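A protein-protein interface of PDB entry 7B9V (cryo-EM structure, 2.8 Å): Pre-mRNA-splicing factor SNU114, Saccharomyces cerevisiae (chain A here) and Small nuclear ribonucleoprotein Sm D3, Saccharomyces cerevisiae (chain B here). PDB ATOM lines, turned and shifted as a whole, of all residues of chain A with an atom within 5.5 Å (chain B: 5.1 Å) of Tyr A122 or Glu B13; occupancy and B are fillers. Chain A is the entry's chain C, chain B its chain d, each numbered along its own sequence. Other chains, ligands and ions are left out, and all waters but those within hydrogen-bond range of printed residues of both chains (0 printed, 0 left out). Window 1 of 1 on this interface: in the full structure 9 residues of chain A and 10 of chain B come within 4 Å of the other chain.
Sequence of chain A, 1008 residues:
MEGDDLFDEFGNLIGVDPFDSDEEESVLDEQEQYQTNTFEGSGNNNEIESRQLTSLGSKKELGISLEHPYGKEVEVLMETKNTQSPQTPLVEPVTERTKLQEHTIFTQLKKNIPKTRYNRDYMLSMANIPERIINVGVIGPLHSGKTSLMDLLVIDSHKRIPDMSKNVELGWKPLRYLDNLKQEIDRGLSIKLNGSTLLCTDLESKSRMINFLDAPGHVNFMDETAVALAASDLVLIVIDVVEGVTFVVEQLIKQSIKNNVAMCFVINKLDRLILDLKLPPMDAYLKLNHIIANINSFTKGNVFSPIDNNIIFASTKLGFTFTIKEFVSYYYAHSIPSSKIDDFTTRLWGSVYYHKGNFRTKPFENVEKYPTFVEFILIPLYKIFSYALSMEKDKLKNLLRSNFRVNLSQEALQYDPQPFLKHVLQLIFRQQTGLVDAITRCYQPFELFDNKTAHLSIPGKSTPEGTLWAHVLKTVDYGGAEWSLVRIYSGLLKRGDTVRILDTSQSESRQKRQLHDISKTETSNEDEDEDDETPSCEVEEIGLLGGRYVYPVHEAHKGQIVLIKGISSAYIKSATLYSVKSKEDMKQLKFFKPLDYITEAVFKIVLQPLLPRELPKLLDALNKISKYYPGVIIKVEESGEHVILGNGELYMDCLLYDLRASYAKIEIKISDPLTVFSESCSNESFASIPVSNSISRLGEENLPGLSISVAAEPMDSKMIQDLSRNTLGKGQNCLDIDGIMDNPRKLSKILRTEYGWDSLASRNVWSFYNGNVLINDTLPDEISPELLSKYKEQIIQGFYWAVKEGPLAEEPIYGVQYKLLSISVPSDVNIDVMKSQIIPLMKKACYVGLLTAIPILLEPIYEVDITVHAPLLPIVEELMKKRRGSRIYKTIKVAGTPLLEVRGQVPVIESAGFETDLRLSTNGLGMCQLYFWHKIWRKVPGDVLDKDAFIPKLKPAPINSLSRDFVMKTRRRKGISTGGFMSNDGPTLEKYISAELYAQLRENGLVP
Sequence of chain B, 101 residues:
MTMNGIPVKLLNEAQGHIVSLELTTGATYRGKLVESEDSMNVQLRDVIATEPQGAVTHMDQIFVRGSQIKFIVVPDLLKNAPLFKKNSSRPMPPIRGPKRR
Of chain B, only Glu B13, Ala B81 and Pro B82 come within 4 Å of Tyr A122. Glu B13 touches just these residues of chain A: Tyr A122 (2.6 Å), Met A126 (3.8 Å), Arg A132 (2.5 Å), Ser A205 (3.4 Å), Lys A206 (3.5 Å) and Ser A207 (2.8 Å). Of the printed residues of chain B, Ser A207 touches Glu B13 (2.8 Å) and Pro B82 (3.4 Å). Of the printed residues of chain B, Ser A205 touches Lys B9 and Glu B13. Of the printed residues of chain B, Met A126 touches Glu B13 (3.8 Å). Ser A125 touches none of the printed residues of chain B. Leu B10 touches none of the printed residues of chain A. The nearest residue of chain B that does not touch Tyr A122 is Leu B78 (4.03 Å). The nearest printed residue of chain A that does not touch Glu B13 is Leu A199 (6.5 Å).
Among the printed residues, merely in contact across the chains: Tyr A122 with Ala B81 (3.6 Å), Tyr A122 with Pro B82 (3.7 Å), Met A126 with Glu B13 (3.8 Å), Arg A132 with Ala B14 (3.96 Å), Lys A206 with Asn B12 (3.7 Å), Lys A206 with Glu B13 (3.5 Å) and Ser A207 with Pro B82 (3.4 Å).
Hydrophobic or aromatic side chains of chain A within 4 Å of the printed part of chain B: Tyr A122 and Met A126. Hydrophobic or aromatic side chains of chain B that line the printed part of chain A: Ala B81 and Pro B82.
The side-chain amino group of Lys B9 is in hydrogen-bond range of the side-chain hydroxyl of Ser A205. The side-chain hydroxyl (OH) of Tyr A122 is in hydrogen-bond range of the side-chain carboxylate (OE2) of Glu B13, at 2.6 Å. NH1 of Arg A132 lies within salt-bridge range of OE2 of Glu B13 (2.8 Å). The side-chain carboxylate of Glu B13 sits at hydrogen-bond distance from the backbone NH of Ser A207, at 2.8 Å. NH2 of Arg A132 lies within hydrogen-bond range of O of Gln B15 (2.9 Å). The side-chain amide oxygen (OE1) of Gln B15 sits at hydrogen-bond distance from the side-chain amino group (NZ) of Lys A206 (2.8 Å). The backbone carbonyl oxygen (O) of Ser A205 lies close to the side-chain carboxylate (OE1) of Glu B13 (3.4 Å).
The side-chain amide oxygen of Asn B12 sits at hydrogen-bond distance from the side-chain amide nitrogen of Gln B15, 3.4 Å away. The backbone carbonyl oxygen (O) of Ala B14 is in hydrogen-bond range of a ring nitrogen (ND1) of His B17 (3.4 Å). N of Tyr A122 is in hydrogen-bond range of OD1 of Asn A119, at 3.0 Å. The side-chain hydroxyl of Ser A125 lies within hydrogen-bond range of the backbone carbonyl oxygen of Tyr A122, 2.7 Å away. NH1 of Arg A132 sits at hydrogen-bond distance from O of Ser A207, at 2.8 Å.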
ATOM      1  N   ASN A 119       3.741  15.691 -22.015  1.00  0.00           N
ATOM      2  CA  ASN A 119       3.235  15.777 -23.378  1.00  0.00           C
ATOM      3  C   ASN A 119       1.716  15.658 -23.347  1.00  0.00           C
ATOM      4  O   ASN A 119       1.180  14.682 -22.813  1.00  0.00           O
ATOM      5  CB  ASN A 119       3.846  14.681 -24.246  1.00  0.00           C
ATOM      6  CG  ASN A 119       3.374  14.751 -25.680  1.00  0.00           C
ATOM      7  OD1 ASN A 119       2.383  14.122 -26.050  1.00  0.00           O
ATOM      8  ND2 ASN A 119       4.073  15.532 -26.496  1.00  0.00           N
ATOM      9  N   ARG A 120       1.021  16.657 -23.904  1.00  0.00           N
ATOM     10  CA  ARG A 120      -0.433  16.710 -23.767  1.00  0.00           C
ATOM     11  C   ARG A 120      -1.128  15.676 -24.647  1.00  0.00           C
ATOM     12  O   ARG A 120      -2.233  15.230 -24.303  1.00  0.00           O
ATOM     13  CB  ARG A 120      -0.951  18.117 -24.080  1.00  0.00           C
ATOM     14  CG  ARG A 120      -2.323  18.391 -23.474  1.00  0.00           C
ATOM     15  CD  ARG A 120      -2.952  19.681 -23.937  1.00  0.00           C
ATOM     16  NE  ARG A 120      -2.708  20.797 -23.030  1.00  0.00           N
ATOM     17  CZ  ARG A 120      -1.876  21.800 -23.273  1.00  0.00           C
ATOM     18  NH1 ARG A 120      -1.183  21.866 -24.399  1.00  0.00           N
ATOM     19  NH2 ARG A 120      -1.755  22.772 -22.376  1.00  0.00           N
ATOM     20  N   ASP A 121      -0.542  15.340 -25.809  1.00  0.00           N
ATOM     21  CA  ASP A 121      -1.136  14.324 -26.684  1.00  0.00           C
ATOM     22  C   ASP A 121      -1.179  12.969 -25.989  1.00  0.00           C
ATOM     23  O   ASP A 121      -2.100  12.171 -26.219  1.00  0.00           O
ATOM     24  CB  ASP A 121      -0.357  14.227 -27.995  1.00  0.00           C
ATOM     25  CG  ASP A 121      -0.414  15.509 -28.806  1.00  0.00           C
ATOM     26  OD1 ASP A 121      -0.773  16.560 -28.240  1.00  0.00           O
ATOM     27  OD2 ASP A 121      -0.102  15.458 -30.017  1.00  0.00           O
ATOM     28  N   TYR A 122      -0.154  12.673 -25.182  1.00  0.00           N
ATOM     29  CA  TYR A 122      -0.115  11.450 -24.383  1.00  0.00           C
ATOM     30  C   TYR A 122      -1.290  11.344 -23.417  1.00  0.00           C
ATOM     31  O   TYR A 122      -1.830  10.251 -23.192  1.00  0.00           O
ATOM     32  CB  TYR A 122       1.200  11.314 -23.622  1.00  0.00           C
ATOM     33  CG  TYR A 122       1.193  10.035 -22.822  1.00  0.00           C
ATOM     34  CD1 TYR A 122       1.131   8.802 -23.461  1.00  0.00           C
ATOM     35  CD2 TYR A 122       1.224  10.065 -21.431  1.00  0.00           C
ATOM     36  CE1 TYR A 122       1.132   7.626 -22.737  1.00  0.00           C
ATOM     37  CE2 TYR A 122       1.211   8.899 -20.700  1.00  0.00           C
ATOM     38  CZ  TYR A 122       1.170   7.681 -21.359  1.00  0.00           C
ATOM     39  OH  TYR A 122       1.121   6.517 -20.635  1.00  0.00           O
ATOM     40  N   MET A 123      -1.676  12.473 -22.815  1.00  0.00           N
ATOM     41  CA  MET A 123      -2.864  12.524 -21.967  1.00  0.00           C
ATOM     42  C   MET A 123      -4.133  12.195 -22.752  1.00  0.00           C
ATOM     43  O   MET A 123      -5.006  11.478 -22.246  1.00  0.00           O
ATOM     44  CB  MET A 123      -2.967  13.893 -21.294  1.00  0.00           C
ATOM     45  CG  MET A 123      -4.070  13.974 -20.244  1.00  0.00           C
ATOM     46  SD  MET A 123      -4.373  15.610 -19.551  1.00  0.00           S
ATOM     47  CE  MET A 123      -4.968  16.492 -20.992  1.00  0.00           C
ATOM     48  N   LEU A 124      -4.305  12.796 -23.935  1.00  0.00           N
ATOM     49  CA  LEU A 124      -5.422  12.432 -24.813  1.00  0.00           C
ATOM     50  C   LEU A 124      -5.391  10.957 -25.213  1.00  0.00           C
ATOM     51  O   LEU A 124      -6.447  10.339 -25.387  1.00  0.00           O
ATOM     52  CB  LEU A 124      -5.415  13.300 -26.068  1.00  0.00           C
ATOM     53  CG  LEU A 124      -5.344  14.812 -25.935  1.00  0.00           C
ATOM     54  CD1 LEU A 124      -5.428  15.460 -27.311  1.00  0.00           C
ATOM     55  CD2 LEU A 124      -6.465  15.301 -25.050  1.00  0.00           C
ATOM     56  N   SER A 125      -4.195  10.412 -25.490  1.00  0.00           N
ATOM     57  CA  SER A 125      -4.059   9.025 -25.946  1.00  0.00           C
ATOM     58  C   SER A 125      -4.552   7.994 -24.928  1.00  0.00           C
ATOM     59  O   SER A 125      -4.903   6.876 -25.321  1.00  0.00           O
ATOM     60  CB  SER A 125      -2.597   8.741 -26.292  1.00  0.00           C
ATOM     61  OG  SER A 125      -1.848   8.424 -25.129  1.00  0.00           O
ATOM     62  N   MET A 126      -4.597   8.343 -23.641  1.00  0.00           N
ATOM     63  CA  MET A 126      -5.172   7.488 -22.611  1.00  0.00           C
ATOM     64  C   MET A 126      -6.606   7.855 -22.236  1.00  0.00           C
ATOM     65  O   MET A 126      -7.190   7.177 -21.388  1.00  0.00           O
ATOM     66  CB  MET A 126      -4.288   7.459 -21.360  1.00  0.00           C
ATOM     67  CG  MET A 126      -4.248   8.732 -20.550  1.00  0.00           C
ATOM     68  SD  MET A 126      -3.641   8.370 -18.892  1.00  0.00           S
ATOM     69  CE  MET A 126      -1.941   7.958 -19.268  1.00  0.00           C
ATOM     70  N   ARG A 132      -8.257   4.695 -16.745  1.00  0.00           N
ATOM     71  CA  ARG A 132      -7.258   5.736 -16.521  1.00  0.00           C
ATOM     72  C   ARG A 132      -7.829   7.114 -16.210  1.00  0.00           C
ATOM     73  O   ARG A 132      -7.051   8.050 -16.027  1.00  0.00           O
ATOM     74  CB  ARG A 132      -6.366   5.851 -17.756  1.00  0.00           C
ATOM     75  CG  ARG A 132      -5.439   4.682 -17.953  1.00  0.00           C
ATOM     76  CD  ARG A 132      -4.453   4.516 -16.833  1.00  0.00           C
ATOM     77  NE  ARG A 132      -3.433   3.570 -17.270  1.00  0.00           N
ATOM     78  CZ  ARG A 132      -2.245   3.906 -17.749  1.00  0.00           C
ATOM     79  NH1 ARG A 132      -1.645   5.029 -17.381  1.00  0.00           N
ATOM     80  NH2 ARG A 132      -1.586   3.028 -18.500  1.00  0.00           N
ATOM     81  N   LEU A 199      -2.837  15.595 -16.470  1.00  0.00           N
ATOM     82  CA  LEU A 199      -2.124  14.325 -16.326  1.00  0.00           C
ATOM     83  C   LEU A 199      -1.375  14.300 -14.995  1.00  0.00           C
ATOM     84  O   LEU A 199      -0.466  15.105 -14.765  1.00  0.00           O
ATOM     85  CB  LEU A 199      -1.172  14.090 -17.494  1.00  0.00           C
ATOM     86  CG  LEU A 199      -0.554  12.693 -17.550  1.00  0.00           C
ATOM     87  CD1 LEU A 199      -1.545  11.705 -18.132  1.00  0.00           C
ATOM     88  CD2 LEU A 199       0.707  12.705 -18.394  1.00  0.00           C
ATOM     89  N   SER A 205       4.821   5.972 -10.013  1.00  0.00           N
ATOM     90  CA  SER A 205       5.036   6.543 -11.350  1.00  0.00           C
ATOM     91  C   SER A 205       3.952   6.231 -12.392  1.00  0.00           C
ATOM     92  O   SER A 205       4.153   6.541 -13.570  1.00  0.00           O
ATOM     93  CB  SER A 205       6.423   6.221 -11.930  1.00  0.00           C
ATOM     94  OG  SER A 205       7.428   6.450 -10.950  1.00  0.00           O
ATOM     95  N   LYS A 206       2.817   5.638 -12.012  1.00  0.00           N
ATOM     96  CA  LYS A 206       1.733   5.415 -12.973  1.00  0.00           C
ATOM     97  C   LYS A 206       0.869   6.669 -13.150  1.00  0.00           C
ATOM     98  O   LYS A 206       0.525   7.350 -12.178  1.00  0.00           O
ATOM     99  CB  LYS A 206       0.878   4.217 -12.544  1.00  0.00           C
ATOM    100  CG  LYS A 206      -0.243   3.844 -13.522  1.00  0.00           C
ATOM    101  CD  LYS A 206      -1.047   2.632 -13.071  1.00  0.00           C
ATOM    102  CE  LYS A 206      -2.288   2.460 -13.939  1.00  0.00           C
ATOM    103  NZ  LYS A 206      -3.282   1.531 -13.337  1.00  0.00           N
ATOM    104  N   SER A 207       0.513   6.965 -14.403  1.00  0.00           N
ATOM    105  CA  SER A 207      -0.211   8.173 -14.788  1.00  0.00           C
ATOM    106  C   SER A 207      -1.716   7.970 -14.965  1.00  0.00           C
ATOM    107  O   SER A 207      -2.163   6.919 -15.436  1.00  0.00           O
ATOM    108  CB  SER A 207       0.355   8.718 -16.096  1.00  0.00           C
ATOM    109  OG  SER A 207       1.765   8.754 -16.055  1.00  0.00           O
ATOM    110  N   LYS B   9       7.642  -0.442 -13.818  1.00  0.00           N
ATOM    111  CA  LYS B   9       6.819   0.764 -13.894  1.00  0.00           C
ATOM    112  C   LYS B   9       6.177   0.926 -15.275  1.00  0.00           C
ATOM    113  O   LYS B   9       5.053   1.422 -15.380  1.00  0.00           O
ATOM    114  CB  LYS B   9       7.629   2.000 -13.511  1.00  0.00           C
ATOM    115  CG  LYS B   9       8.010   2.099 -12.034  1.00  0.00           C
ATOM    116  CD  LYS B   9       8.937   3.283 -11.793  1.00  0.00           C
ATOM    117  CE  LYS B   9       9.122   3.541 -10.308  1.00  0.00           C
ATOM    118  NZ  LYS B   9       9.945   4.752 -10.054  1.00  0.00           N
ATOM    119  N   LEU B  10       6.892   0.561 -16.344  1.00  0.00           N
ATOM    120  CA  LEU B  10       6.348   0.592 -17.705  1.00  0.00           C
ATOM    121  C   LEU B  10       5.243  -0.434 -17.896  1.00  0.00           C
ATOM    122  O   LEU B  10       4.249  -0.163 -18.586  1.00  0.00           O
ATOM    123  CB  LEU B  10       7.473   0.394 -18.722  1.00  0.00           C
ATOM    124  CG  LEU B  10       7.103   0.431 -20.205  1.00  0.00           C
ATOM    125  CD1 LEU B  10       6.586   1.806 -20.581  1.00  0.00           C
ATOM    126  CD2 LEU B  10       8.312   0.080 -21.050  1.00  0.00           C
ATOM    127  N   LEU B  11       5.397  -1.611 -17.296  1.00  0.00           N
ATOM    128  CA  LEU B  11       4.324  -2.606 -17.324  1.00  0.00           C
ATOM    129  C   LEU B  11       3.103  -2.169 -16.511  1.00  0.00           C
ATOM    130  O   LEU B  11       1.964  -2.468 -16.896  1.00  0.00           O
ATOM    131  CB  LEU B  11       4.857  -3.959 -16.848  1.00  0.00           C
ATOM    132  CG  LEU B  11       3.872  -5.123 -16.918  1.00  0.00           C
ATOM    133  CD1 LEU B  11       3.479  -5.341 -18.361  1.00  0.00           C
ATOM    134  CD2 LEU B  11       4.507  -6.369 -16.335  1.00  0.00           C
ATOM    135  N   ASN B  12       3.301  -1.377 -15.458  1.00  0.00           N
ATOM    136  CA  ASN B  12       2.148  -0.769 -14.781  1.00  0.00           C
ATOM    137  C   ASN B  12       1.519   0.363 -15.602  1.00  0.00           C
ATOM    138  O   ASN B  12       0.288   0.452 -15.692  1.00  0.00           O
ATOM    139  CB  ASN B  12       2.565  -0.296 -13.393  1.00  0.00           C
ATOM    140  CG  ASN B  12       2.553  -1.427 -12.379  1.00  0.00           C
ATOM    141  OD1 ASN B  12       1.543  -1.678 -11.728  1.00  0.00           O
ATOM    142  ND2 ASN B  12       3.663  -2.137 -12.279  1.00  0.00           N
ATOM    143  N   GLU B  13       2.339   1.225 -16.213  1.00  0.00           N
ATOM    144  CA  GLU B  13       1.961   2.298 -17.147  1.00  0.00           C
ATOM    145  C   GLU B  13       1.407   1.755 -18.474  1.00  0.00           C
ATOM    146  O   GLU B  13       0.790   2.506 -19.238  1.00  0.00           O
ATOM    147  CB  GLU B  13       3.181   3.223 -17.363  1.00  0.00           C
ATOM    148  CG  GLU B  13       2.989   4.543 -18.136  1.00  0.00           C
ATOM    149  CD  GLU B  13       1.995   5.480 -17.486  1.00  0.00           C
ATOM    150  OE1 GLU B  13       2.256   5.951 -16.359  1.00  0.00           O
ATOM    151  OE2 GLU B  13       0.948   5.748 -18.116  1.00  0.00           O
ATOM    152  N   ALA B  14       1.486   0.447 -18.702  1.00  0.00           N
ATOM    153  CA  ALA B  14       0.819  -0.196 -19.828  1.00  0.00           C
ATOM    154  C   ALA B  14      -0.610  -0.659 -19.561  1.00  0.00           C
ATOM    155  O   ALA B  14      -1.254  -1.074 -20.533  1.00  0.00           O
ATOM    156  CB  ALA B  14       1.630  -1.407 -20.298  1.00  0.00           C
ATOM    157  N   GLN B  15      -1.059  -0.745 -18.293  1.00  0.00           N
ATOM    158  CA  GLN B  15      -2.404  -1.239 -17.970  1.00  0.00           C
ATOM    159  C   GLN B  15      -3.488  -0.437 -18.690  1.00  0.00           C
ATOM    160  O   GLN B  15      -3.430   0.796 -18.768  1.00  0.00           O
ATOM    161  CB  GLN B  15      -2.680  -1.202 -16.463  1.00  0.00           C
ATOM    162  CG  GLN B  15      -1.886  -2.196 -15.606  1.00  0.00           C
ATOM    163  CD  GLN B  15      -2.111  -2.000 -14.095  1.00  0.00           C
ATOM    164  OE1 GLN B  15      -2.974  -1.238 -13.680  1.00  0.00           O
ATOM    165  NE2 GLN B  15      -1.302  -2.671 -13.294  1.00  0.00           N
ATOM    166  N   HIS B  17      -4.048  -0.759 -21.943  1.00  0.00           N
ATOM    167  CA  HIS B  17      -3.747  -0.941 -23.363  1.00  0.00           C
ATOM    168  C   HIS B  17      -3.680  -2.423 -23.767  1.00  0.00           C
ATOM    169  O   HIS B  17      -3.595  -3.333 -22.937  1.00  0.00           O
ATOM    170  CB  HIS B  17      -2.430  -0.293 -23.775  1.00  0.00           C
ATOM    171  CG  HIS B  17      -2.348   1.193 -23.563  1.00  0.00           C
ATOM    172  ND1 HIS B  17      -1.992   1.762 -22.351  1.00  0.00           N
ATOM    173  CD2 HIS B  17      -2.470   2.222 -24.439  1.00  0.00           C
ATOM    174  CE1 HIS B  17      -1.964   3.073 -22.482  1.00  0.00           C
ATOM    175  NE2 HIS B  17      -2.249   3.379 -23.742  1.00  0.00           N
ATOM    176  N   LEU B  77       3.207   4.275 -28.279  1.00  0.00           N
ATOM    177  CA  LEU B  77       2.883   5.596 -27.739  1.00  0.00           C
ATOM    178  C   LEU B  77       3.658   5.880 -26.461  1.00  0.00           C
ATOM    179  O   LEU B  77       4.018   7.032 -26.192  1.00  0.00           O
ATOM    180  CB  LEU B  77       1.394   5.664 -27.426  1.00  0.00           C
ATOM    181  CG  LEU B  77       0.407   5.401 -28.553  1.00  0.00           C
ATOM    182  CD1 LEU B  77      -1.005   5.296 -27.987  1.00  0.00           C
ATOM    183  CD2 LEU B  77       0.501   6.500 -29.581  1.00  0.00           C
ATOM    184  N   LEU B  78       3.916   4.837 -25.667  1.00  0.00           N
ATOM    185  CA  LEU B  78       4.466   4.971 -24.326  1.00  0.00           C
ATOM    186  C   LEU B  78       5.914   5.451 -24.299  1.00  0.00           C
ATOM    187  O   LEU B  78       6.429   5.680 -23.200  1.00  0.00           O
ATOM    188  CB  LEU B  78       4.268   3.673 -23.524  1.00  0.00           C
ATOM    189  CG  LEU B  78       2.910   3.557 -22.775  1.00  0.00           C
ATOM    190  CD1 LEU B  78       1.600   3.705 -23.560  1.00  0.00           C
ATOM    191  CD2 LEU B  78       2.852   2.314 -21.892  1.00  0.00           C
ATOM    192  N   ASN B  80       6.989   8.226 -25.071  1.00  0.00           N
ATOM    193  CA  ASN B  80       6.908   9.601 -24.606  1.00  0.00           C
ATOM    194  C   ASN B  80       6.076   9.748 -23.335  1.00  0.00           C
ATOM    195  O   ASN B  80       5.663  10.865 -23.014  1.00  0.00           O
ATOM    196  CB  ASN B  80       6.329  10.475 -25.720  1.00  0.00           C
ATOM    197  CG  ASN B  80       7.252  10.575 -26.918  1.00  0.00           C
ATOM    198  OD1 ASN B  80       6.967  10.025 -27.984  1.00  0.00           O
ATOM    199  ND2 ASN B  80       8.376  11.256 -26.743  1.00  0.00           N
ATOM    200  N   ALA B  81       5.781   8.654 -22.629  1.00  0.00           N
ATOM    201  CA  ALA B  81       5.142   8.740 -21.317  1.00  0.00           C
ATOM    202  C   ALA B  81       6.067   9.415 -20.290  1.00  0.00           C
ATOM    203  O   ALA B  81       7.292   9.358 -20.436  1.00  0.00           O
ATOM    204  CB  ALA B  81       4.766   7.324 -20.862  1.00  0.00           C
ATOM    205  N   PRO B  82       5.512  10.061 -19.245  1.00  0.00           N
ATOM    206  CA  PRO B  82       6.360  10.798 -18.276  1.00  0.00           C
ATOM    207  C   PRO B  82       7.320   9.949 -17.438  1.00  0.00           C
ATOM    208  O   PRO B  82       8.160  10.520 -16.732  1.00  0.00           O
ATOM    209  CB  PRO B  82       5.343  11.525 -17.379  1.00  0.00           C
ATOM    210  CG  PRO B  82       4.170  10.676 -17.384  1.00  0.00           C
ATOM    211  CD  PRO B  82       4.106  10.220 -18.849  1.00  0.00           C
ATOM    212  N   LEU B  83       7.161   8.629 -17.467  1.00  0.00           N
ATOM    213  CA  LEU B  83       8.041   7.656 -16.826  1.00  0.00           C
ATOM    214  C   LEU B  83       9.519   7.799 -17.202  1.00  0.00           C
ATOM    215  O   LEU B  83      10.402   7.692 -16.337  1.00  0.00           O
ATOM    216  CB  LEU B  83       7.554   6.270 -17.207  1.00  0.00           C
ATOM    217  CG  LEU B  83       8.411   5.120 -16.743  1.00  0.00           C
ATOM    218  CD1 LEU B  83       8.460   5.125 -15.220  1.00  0.00           C
ATOM    219  CD2 LEU B  83       7.794   3.903 -17.268  1.00  0.00           C
